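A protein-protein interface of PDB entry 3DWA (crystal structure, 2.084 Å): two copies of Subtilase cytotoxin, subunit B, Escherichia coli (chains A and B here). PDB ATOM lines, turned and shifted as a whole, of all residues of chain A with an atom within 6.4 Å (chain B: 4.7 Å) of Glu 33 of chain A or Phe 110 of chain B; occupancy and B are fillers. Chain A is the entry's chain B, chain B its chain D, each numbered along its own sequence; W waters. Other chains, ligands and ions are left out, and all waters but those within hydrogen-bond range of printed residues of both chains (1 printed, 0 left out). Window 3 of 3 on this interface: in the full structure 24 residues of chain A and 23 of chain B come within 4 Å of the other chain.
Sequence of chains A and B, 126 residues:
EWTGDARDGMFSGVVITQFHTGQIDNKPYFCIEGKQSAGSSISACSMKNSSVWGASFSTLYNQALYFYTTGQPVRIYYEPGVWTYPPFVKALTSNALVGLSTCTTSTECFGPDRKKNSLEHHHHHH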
ATOM      1  N   VAL A  14      -5.799   2.861   4.903  1.00  0.00           N
ATOM      2  CA  VAL A  14      -4.732   3.826   4.600  1.00  0.00           C
ATOM      3  C   VAL A  14      -3.600   3.860   5.646  1.00  0.00           C
ATOM      4  O   VAL A  14      -3.865   3.928   6.849  1.00  0.00           O
ATOM      5  CB  VAL A  14      -5.349   5.228   4.470  1.00  0.00           C
ATOM      6  CG1 VAL A  14      -4.261   6.280   4.516  1.00  0.00           C
ATOM      7  CG2 VAL A  14      -6.103   5.301   3.219  1.00  0.00           C
ATOM      8  N   VAL A  15      -2.343   3.771   5.192  1.00  0.00           N
ATOM      9  CA  VAL A  15      -1.228   4.136   6.046  1.00  0.00           C
ATOM     10  C   VAL A  15      -0.925   5.665   5.924  1.00  0.00           C
ATOM     11  O   VAL A  15      -0.679   6.173   4.824  1.00  0.00           O
ATOM     12  CB  VAL A  15       0.055   3.265   5.774  1.00  0.00           C
ATOM     13  CG1 VAL A  15       1.247   3.721   6.638  1.00  0.00           C
ATOM     14  CG2 VAL A  15      -0.211   1.704   5.947  1.00  0.00           C
ATOM     15  N   ILE A  16      -0.971   6.377   7.054  1.00  0.00           N
ATOM     16  CA  ILE A  16      -0.621   7.813   7.113  1.00  0.00           C
ATOM     17  C   ILE A  16       0.873   7.938   7.084  1.00  0.00           C
ATOM     18  O   ILE A  16       1.524   7.431   7.957  1.00  0.00           O
ATOM     19  CB  ILE A  16      -1.185   8.541   8.379  1.00  0.00           C
ATOM     20  CG1 ILE A  16      -2.732   8.468   8.432  1.00  0.00           C
ATOM     21  CG2 ILE A  16      -0.624   9.969   8.436  1.00  0.00           C
ATOM     22  CD1 ILE A  16      -3.403   8.996   9.736  1.00  0.00           C
ATOM     23  N   THR A  17       1.408   8.579   6.030  1.00  0.00           N
ATOM     24  CA  THR A  17       2.839   8.596   5.727  1.00  0.00           C
ATOM     25  C   THR A  17       3.429   9.987   5.748  1.00  0.00           C
ATOM     26  O   THR A  17       4.648  10.118   5.754  1.00  0.00           O
ATOM     27  CB  THR A  17       3.130   8.066   4.293  1.00  0.00           C
ATOM     28  OG1 THR A  17       2.181   8.644   3.385  1.00  0.00           O
ATOM     29  CG2 THR A  17       2.983   6.535   4.236  1.00  0.00           C
ATOM     30  N   GLN A  18       2.584  11.022   5.705  1.00  0.00           N
ATOM     31  CA  GLN A  18       3.102  12.388   5.724  1.00  0.00           C
ATOM     32  C   GLN A  18       2.243  13.231   6.621  1.00  0.00           C
ATOM     33  O   GLN A  18       1.068  12.986   6.748  1.00  0.00           O
ATOM     34  CB  GLN A  18       3.203  13.015   4.297  1.00  0.00           C
ATOM     35  CG  GLN A  18       4.000  12.158   3.238  1.00  0.00           C
ATOM     36  CD  GLN A  18       5.534  12.039   3.517  1.00  0.00           C
ATOM     37  OE1 GLN A  18       6.130  10.994   3.238  1.00  0.00           O
ATOM     38  NE2 GLN A  18       6.158  13.091   4.065  1.00  0.00           N
ATOM     39  N   PHE A  19       2.856  14.226   7.237  1.00  0.00           N
ATOM     40  CA  PHE A  19       2.201  15.056   8.208  1.00  0.00           C
ATOM     41  C   PHE A  19       2.695  16.485   7.990  1.00  0.00           C
ATOM     42  O   PHE A  19       3.884  16.673   7.901  1.00  0.00           O
ATOM     43  CB  PHE A  19       2.566  14.578   9.635  1.00  0.00           C
ATOM     44  CG  PHE A  19       1.470  14.795  10.625  1.00  0.00           C
ATOM     45  CD1 PHE A  19       0.663  13.732  11.013  1.00  0.00           C
ATOM     46  CD2 PHE A  19       1.226  16.085  11.157  1.00  0.00           C
ATOM     47  CE1 PHE A  19      -0.369  13.906  11.908  1.00  0.00           C
ATOM     48  CE2 PHE A  19       0.180  16.287  12.083  1.00  0.00           C
ATOM     49  CZ  PHE A  19      -0.623  15.181  12.457  1.00  0.00           C
ATOM     50  N   HIS A  20       1.784  17.458   7.860  1.00  0.00           N
ATOM     51  CA  HIS A  20       2.161  18.884   7.703  1.00  0.00           C
ATOM     52  C   HIS A  20       1.328  19.710   8.676  1.00  0.00           C
ATOM     53  O   HIS A  20       0.191  19.401   8.940  1.00  0.00           O
ATOM     54  CB  HIS A  20       1.957  19.413   6.253  1.00  0.00           C
ATOM     55  CG  HIS A  20       2.033  20.914   6.129  1.00  0.00           C
ATOM     56  ND1 HIS A  20       0.930  21.700   5.824  1.00  0.00           N
ATOM     57  CD2 HIS A  20       3.078  21.768   6.245  1.00  0.00           C
ATOM     58  CE1 HIS A  20       1.286  22.970   5.821  1.00  0.00           C
ATOM     59  NE2 HIS A  20       2.586  23.035   6.059  1.00  0.00           N
ATOM     60  N   CYS A  31      -2.310  18.702   7.998  1.00  0.00           N
ATOM     61  CA  CYS A  31      -2.727  17.949   6.839  1.00  0.00           C
ATOM     62  C   CYS A  31      -1.975  16.618   6.883  1.00  0.00           C
ATOM     63  O   CYS A  31      -0.825  16.560   7.339  1.00  0.00           O
ATOM     64  CB  CYS A  31      -2.508  18.776   5.530  1.00  0.00           C
ATOM     65  SG  CYS A  31      -3.724  18.280   4.183  1.00  0.00           S
ATOM     66  N   ILE A  32      -2.637  15.549   6.468  1.00  0.00           N
ATOM     67  CA  ILE A  32      -1.991  14.227   6.376  1.00  0.00           C
ATOM     68  C   ILE A  32      -2.148  13.688   4.970  1.00  0.00           C
ATOM     69  O   ILE A  32      -3.089  14.041   4.256  1.00  0.00           O
ATOM     70  CB  ILE A  32      -2.618  13.199   7.310  1.00  0.00           C
ATOM     71  CG1 ILE A  32      -4.163  13.263   7.201  1.00  0.00           C
ATOM     72  CG2 ILE A  32      -2.122  13.404   8.759  1.00  0.00           C
ATOM     73  CD1 ILE A  32      -4.947  11.971   7.682  1.00  0.00           C
ATOM     74  N   GLU A  33      -1.242  12.803   4.602  1.00  0.00           N
ATOM     75  CA  GLU A  33      -1.324  12.102   3.360  1.00  0.00           C
ATOM     76  C   GLU A  33      -1.137  10.650   3.696  1.00  0.00           C
ATOM     77  O   GLU A  33      -0.232  10.265   4.434  1.00  0.00           O
ATOM     78  CB  GLU A  33      -0.215  12.528   2.386  1.00  0.00           C
ATOM     79  CG  GLU A  33      -0.159  11.651   1.135  1.00  0.00           C
ATOM     80  CD  GLU A  33       1.266  11.288   0.777  1.00  0.00           C
ATOM     81  OE1 GLU A  33       2.131  12.221   0.578  1.00  0.00           O
ATOM     82  OE2 GLU A  33       1.535  10.056   0.716  1.00  0.00           O
ATOM     83  N   GLY A  34      -2.004   9.853   3.133  1.00  0.00           N
ATOM     84  CA  GLY A  34      -1.907   8.428   3.291  1.00  0.00           C
ATOM     85  C   GLY A  34      -1.948   7.740   1.954  1.00  0.00           C
ATOM     86  O   GLY A  34      -2.451   8.291   1.001  1.00  0.00           O
ATOM     87  N   LYS A  35      -1.405   6.541   1.917  1.00  0.00           N
ATOM     88  CA  LYS A  35      -1.487   5.683   0.773  1.00  0.00           C
ATOM     89  C   LYS A  35      -2.350   4.452   1.079  1.00  0.00           C
ATOM     90  O   LYS A  35      -2.168   3.778   2.112  1.00  0.00           O
ATOM     91  CB  LYS A  35      -0.070   5.238   0.389  1.00  0.00           C
ATOM     92  CG  LYS A  35       1.022   6.315   0.431  1.00  0.00           C
ATOM     93  CD  LYS A  35       1.872   6.296  -0.854  1.00  0.00           C
ATOM     94  CE  LYS A  35       2.907   5.151  -0.880  1.00  0.00           C
ATOM     95  NZ  LYS A  35       3.467   4.873  -2.242  1.00  0.00           N
ATOM     96  N   SER A  41      -3.121   7.819  -3.351  1.00  0.00           N
ATOM     97  CA  SER A  41      -3.032   8.731  -2.207  1.00  0.00           C
ATOM     98  C   SER A  41      -4.303   9.520  -1.928  1.00  0.00           C
ATOM     99  O   SER A  41      -5.110   9.817  -2.836  1.00  0.00           O
ATOM    100  CB  SER A  41      -1.896   9.686  -2.414  1.00  0.00           C
ATOM    101  OG  SER A  41      -0.861   8.978  -3.045  1.00  0.00           O
ATOM    102  N   ILE A  42      -4.490   9.832  -0.650  1.00  0.00           N
ATOM    103  CA  ILE A  42      -5.550  10.731  -0.220  1.00  0.00           C
ATOM    104  C   ILE A  42      -4.868  11.779   0.679  1.00  0.00           C
ATOM    105  O   ILE A  42      -3.899  11.490   1.356  1.00  0.00           O
ATOM    106  CB  ILE A  42      -6.718   9.957   0.483  1.00  0.00           C
ATOM    107  CG1 ILE A  42      -7.714  10.911   1.198  1.00  0.00           C
ATOM    108  CG2 ILE A  42      -6.177   8.982   1.573  1.00  0.00           C
ATOM    109  CD1 ILE A  42      -8.830  11.500   0.334  1.00  0.00           C
ATOM    110  N   SER A  43      -5.322  13.006   0.641  1.00  0.00           N
ATOM    111  CA  SER A  43      -4.899  13.978   1.619  1.00  0.00           C
ATOM    112  C   SER A  43      -6.184  14.497   2.233  1.00  0.00           C
ATOM    113  O   SER A  43      -7.210  14.480   1.566  1.00  0.00           O
ATOM    114  CB  SER A  43      -4.149  15.130   0.969  1.00  0.00           C
ATOM    115  OG  SER A  43      -3.307  14.627  -0.025  1.00  0.00           O
ATOM    116  N   ALA A  44      -6.101  14.956   3.480  1.00  0.00           N
ATOM    117  CA  ALA A  44      -7.197  15.615   4.177  1.00  0.00           C
ATOM    118  C   ALA A  44      -6.600  16.552   5.228  1.00  0.00           C
ATOM    119  O   ALA A  44      -5.563  16.221   5.828  1.00  0.00           O
ATOM    120  CB  ALA A  44      -8.081  14.594   4.814  1.00  0.00           C
ATOM    121  N   TYR A  68      -0.133   8.071  12.617  1.00  0.00           N
ATOM    122  CA  TYR A  68       1.145   8.270  11.886  1.00  0.00           C
ATOM    123  C   TYR A  68       2.302   7.510  12.572  1.00  0.00           C
ATOM    124  O   TYR A  68       3.101   6.846  11.919  1.00  0.00           O
ATOM    125  CB  TYR A  68       1.466   9.755  11.765  1.00  0.00           C
ATOM    126  CG  TYR A  68       2.846  10.021  11.189  1.00  0.00           C
ATOM    127  CD1 TYR A  68       3.104   9.916   9.802  1.00  0.00           C
ATOM    128  CD2 TYR A  68       3.878  10.370  12.019  1.00  0.00           C
ATOM    129  CE1 TYR A  68       4.390  10.129   9.278  1.00  0.00           C
ATOM    130  CE2 TYR A  68       5.142  10.598  11.527  1.00  0.00           C
ATOM    131  CZ  TYR A  68       5.385  10.485  10.144  1.00  0.00           C
ATOM    132  OH  TYR A  68       6.657  10.760   9.701  1.00  0.00           O
ATOM    133  N   ALA A  91      -1.673  23.353  -3.299  1.00  0.00           N
ATOM    134  CA  ALA A  91      -0.511  22.789  -2.602  1.00  0.00           C
ATOM    135  C   ALA A  91      -0.875  21.550  -1.787  1.00  0.00           C
ATOM    136  O   ALA A  91      -0.053  20.629  -1.612  1.00  0.00           O
ATOM    137  CB  ALA A  91       0.077  23.836  -1.670  1.00  0.00           C
ATOM    138  N   LEU A  92      -2.096  21.557  -1.274  1.00  0.00           N
ATOM    139  CA  LEU A  92      -2.568  20.574  -0.307  1.00  0.00           C
ATOM    140  C   LEU A  92      -3.820  19.904  -0.824  1.00  0.00           C
ATOM    141  O   LEU A  92      -3.734  18.999  -1.612  1.00  0.00           O
ATOM    142  CB  LEU A  92      -2.784  21.190   1.092  1.00  0.00           C
ATOM    143  CG  LEU A  92      -1.498  21.749   1.736  1.00  0.00           C
ATOM    144  CD1 LEU A  92      -1.822  22.532   2.970  1.00  0.00           C
ATOM    145  CD2 LEU A  92      -0.515  20.618   2.088  1.00  0.00           C
ATOM    146  N   ARG B  75      10.808  19.669   7.257  1.00  0.00           N
ATOM    147  CA  ARG B  75      10.922  20.988   6.675  1.00  0.00           C
ATOM    148  C   ARG B  75      10.551  22.023   7.724  1.00  0.00           C
ATOM    149  O   ARG B  75       9.502  21.866   8.371  1.00  0.00           O
ATOM    150  CB  ARG B  75       9.979  21.105   5.461  1.00  0.00           C
ATOM    151  CG  ARG B  75       9.875  22.512   4.883  1.00  0.00           C
ATOM    152  CD  ARG B  75       9.043  22.414   3.617  1.00  0.00           C
ATOM    153  NE  ARG B  75       9.828  21.856   2.490  1.00  0.00           N
ATOM    154  CZ  ARG B  75       9.315  21.541   1.294  1.00  0.00           C
ATOM    155  NH1 ARG B  75       8.011  21.704   1.052  1.00  0.00           N
ATOM    156  NH2 ARG B  75      10.100  21.044   0.339  1.00  0.00           N
ATOM    157  N   TYR B  77       9.418  25.784   8.079  1.00  0.00           N
ATOM    158  CA  TYR B  77       8.915  27.007   7.480  1.00  0.00           C
ATOM    159  C   TYR B  77       9.103  28.154   8.458  1.00  0.00           C
ATOM    160  O   TYR B  77       8.672  28.078   9.605  1.00  0.00           O
ATOM    161  CB  TYR B  77       7.410  26.900   7.247  1.00  0.00           C
ATOM    162  CG  TYR B  77       7.005  25.901   6.235  1.00  0.00           C
ATOM    163  CD1 TYR B  77       6.862  26.264   4.911  1.00  0.00           C
ATOM    164  CD2 TYR B  77       6.678  24.590   6.616  1.00  0.00           C
ATOM    165  CE1 TYR B  77       6.452  25.330   3.956  1.00  0.00           C
ATOM    166  CE2 TYR B  77       6.269  23.661   5.688  1.00  0.00           C
ATOM    167  CZ  TYR B  77       6.152  24.047   4.346  1.00  0.00           C
ATOM    168  OH  TYR B  77       5.724  23.128   3.411  1.00  0.00           O
ATOM    169  N   SER B 101       6.849  20.181   8.271  1.00  0.00           N
ATOM    170  CA  SER B 101       6.449  19.049   7.416  1.00  0.00           C
ATOM    171  C   SER B 101       7.416  17.899   7.512  1.00  0.00           C
ATOM    172  O   SER B 101       8.602  18.110   7.700  1.00  0.00           O
ATOM    173  CB  SER B 101       6.491  19.468   5.927  1.00  0.00           C
ATOM    174  OG  SER B 101       5.417  20.310   5.578  1.00  0.00           O
ATOM    175  N   THR B 102       6.908  16.682   7.326  1.00  0.00           N
ATOM    176  CA  THR B 102       7.729  15.519   7.151  1.00  0.00           C
ATOM    177  C   THR B 102       8.344  15.579   5.742  1.00  0.00           C
ATOM    178  O   THR B 102       7.802  16.233   4.850  1.00  0.00           O
ATOM    179  CB  THR B 102       6.895  14.233   7.247  1.00  0.00           C
ATOM    180  OG1 THR B 102       5.818  14.332   6.291  1.00  0.00           O
ATOM    181  CG2 THR B 102       6.274  14.059   8.667  1.00  0.00           C
ATOM    182  N   GLU B 108      12.589  16.972  -1.103  1.00  0.00           N
ATOM    183  CA  GLU B 108      11.145  16.702  -1.244  1.00  0.00           C
ATOM    184  C   GLU B 108      10.414  16.430   0.089  1.00  0.00           C
ATOM    185  O   GLU B 108      10.589  15.394   0.712  1.00  0.00           O
ATOM    186  CB  GLU B 108      10.887  15.594  -2.273  1.00  0.00           C
ATOM    187  CG  GLU B 108      11.693  15.830  -3.579  1.00  0.00           C
ATOM    188  CD  GLU B 108      11.035  15.293  -4.834  1.00  0.00           C
ATOM    189  OE1 GLU B 108      10.120  14.423  -4.724  1.00  0.00           O
ATOM    190  OE2 GLU B 108      11.452  15.747  -5.944  1.00  0.00           O
ATOM    191  N   CYS B 109       9.557  17.366   0.479  1.00  0.00           N
ATOM    192  CA  CYS B 109       8.748  17.258   1.688  1.00  0.00           C
ATOM    193  C   CYS B 109       7.262  17.474   1.403  1.00  0.00           C
ATOM    194  O   CYS B 109       6.891  17.949   0.324  1.00  0.00           O
ATOM    195  CB  CYS B 109       9.258  18.272   2.705  1.00  0.00           C
ATOM    196  SG  CYS B 109      11.127  18.226   2.913  1.00  0.00           S
ATOM    197  N   PHE B 110       6.413  17.116   2.365  1.00  0.00           N
ATOM    198  CA  PHE B 110       4.947  17.269   2.250  1.00  0.00           C
ATOM    199  C   PHE B 110       4.551  18.726   2.544  1.00  0.00           C
ATOM    200  O   PHE B 110       5.036  19.316   3.489  1.00  0.00           O
ATOM    201  CB  PHE B 110       4.253  16.301   3.247  1.00  0.00           C
ATOM    202  CG  PHE B 110       2.761  16.267   3.128  1.00  0.00           C
ATOM    203  CD1 PHE B 110       2.157  16.033   1.888  1.00  0.00           C
ATOM    204  CD2 PHE B 110       1.954  16.463   4.257  1.00  0.00           C
ATOM    205  CE1 PHE B 110       0.768  16.005   1.755  1.00  0.00           C
ATOM    206  CE2 PHE B 110       0.590  16.436   4.146  1.00  0.00           C
ATOM    207  CZ  PHE B 110      -0.021  16.218   2.884  1.00  0.00           C
ATOM    208  N   GLY B 111       3.724  19.347   1.717  1.00  0.00           N
ATOM    209  CA  GLY B 111       3.239  20.681   2.058  1.00  0.00           C
ATOM    210  C   GLY B 111       3.509  21.683   0.947  1.00  0.00           C
ATOM    211  O   GLY B 111       4.064  21.315  -0.098  1.00  0.00           O
ATOM    212  N   PRO B 112       3.132  22.952   1.175  1.00  0.00           N
ATOM    213  CA  PRO B 112       3.354  24.037   0.210  1.00  0.00           C
ATOM    214  C   PRO B 112       4.826  24.423   0.153  1.00  0.00           C
ATOM    215  O   PRO B 112       5.578  24.158   1.082  1.00  0.00           O
ATOM    216  CB  PRO B 112       2.559  25.201   0.817  1.00  0.00           C
ATOM    217  CG  PRO B 112       2.661  24.932   2.345  1.00  0.00           C
ATOM    218  CD  PRO B 112       2.477  23.442   2.412  1.00  0.00           C
HETATM  219  O   HOH W   1       2.499  20.382  -2.459  1.00  0.00           O
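N of Thr 102 of chain B lies within hydrogen-bond range of O of Phe 19 of chain A, at 3.1 Å. NE2 of Gln 18 of chain A is in hydrogen-bond range of OG1 of Thr 102 of chain B.
The backbone carbonyl oxygen (O) of Thr 102 of chain B sits at hydrogen-bond distance from the backbone NH (N) of Phe 110 of chain B. O of His 20 of chain A is in hydrogen-bond range of N of Cys 31 of chain A (2.8 Å). N of Arg 75 of chain B lies within hydrogen-bond range of O of Ser 101 of chain B, 2.7 Å away. The backbone carbonyl oxygen (O) of Gln 18 of chain A lies within hydrogen-bond range of the backbone NH (N) of Glu 33 of chain A (3.2 Å). The side-chain hydroxyl (OH) of Tyr 77 of chain B lies within hydrogen-bond range of the backbone carbonyl oxygen (O) of Pro 112 of chain B, at 2.6 Å. N of Thr 17 of chain A is in hydrogen-bond range of O of Glu 33 of chain A (2.8 Å).
Gln 18 of chain A touches Phe 110 of chain B. C of Phe 19 of chain A touches CD2 of Phe 110 of chain B, 3.8 Å away. CD2 of His 20 of chain A touches CE2 of Tyr 77 of chain B (3.8 Å). CD2 of His 20 of chain A touches OG of Ser 101 of chain B, at 2.8 Å. His 20 of chain A touches Phe 110 of chain B (CB to CD2, 3.6 Å). CE1 of His 20 of chain A touches CD of Pro 112 of chain B (3.6 Å). CZ of Phe 110 of chain B touches C of Ile 32 of chain A (3.9 Å). CB of Glu 33 of chain A touches CE1 of Phe 110 of chain B, 3.7 Å away. CB of Pro 112 of chain B touches CB of Ala 91 of chain A, 3.8 Å away. CD2 of Leu 92 of chain A touches CA of Gly 111 of chain B, at 3.8 Å.
Phe 110 of chain B touches six residues of chain A. Printed residues of chain B within 4 Å of Phe 19 of chain A: Ser 101 (3.5 Å), Thr 102 (3.1 Å) and Phe 110 (3.8 Å). Of the printed residues of chain B, Cys 31 of chain A touches Phe 110 (3.5 Å). Ala 44 of chain A touches none of the printed residues of chain B. Cys 109 of chain B touches none of the printed residues of chain A. The nearest residue of chain A that does not touch Phe 110 of chain B is Leu 92 of chain A (4.5 Å). The nearest printed residue of chain A that does not touch Gly 111 of chain B is His 20 of chain A (4.3 Å).
Printed residues of chain A that touch a printed residue of chain B: Gln 18, Phe 19, His 20, Cys 31, Ile 32, Glu 33, Tyr 68, Ala 91 and Leu 92. Of the 9 printed residues of chain B, 6 touch a printed residue of chain A. Among the printed residues, 15 pairs touch across the chains. Among the printed residues, no Asp or Glu carboxylate lies within 4 Å of a Lys or Arg side-chain nitrogen of the other chain.
No position is printed for both chains.
Water W1 lies within hydrogen-bond range of O of Ala 91 of chain A and O of Gly 111 of chain B.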
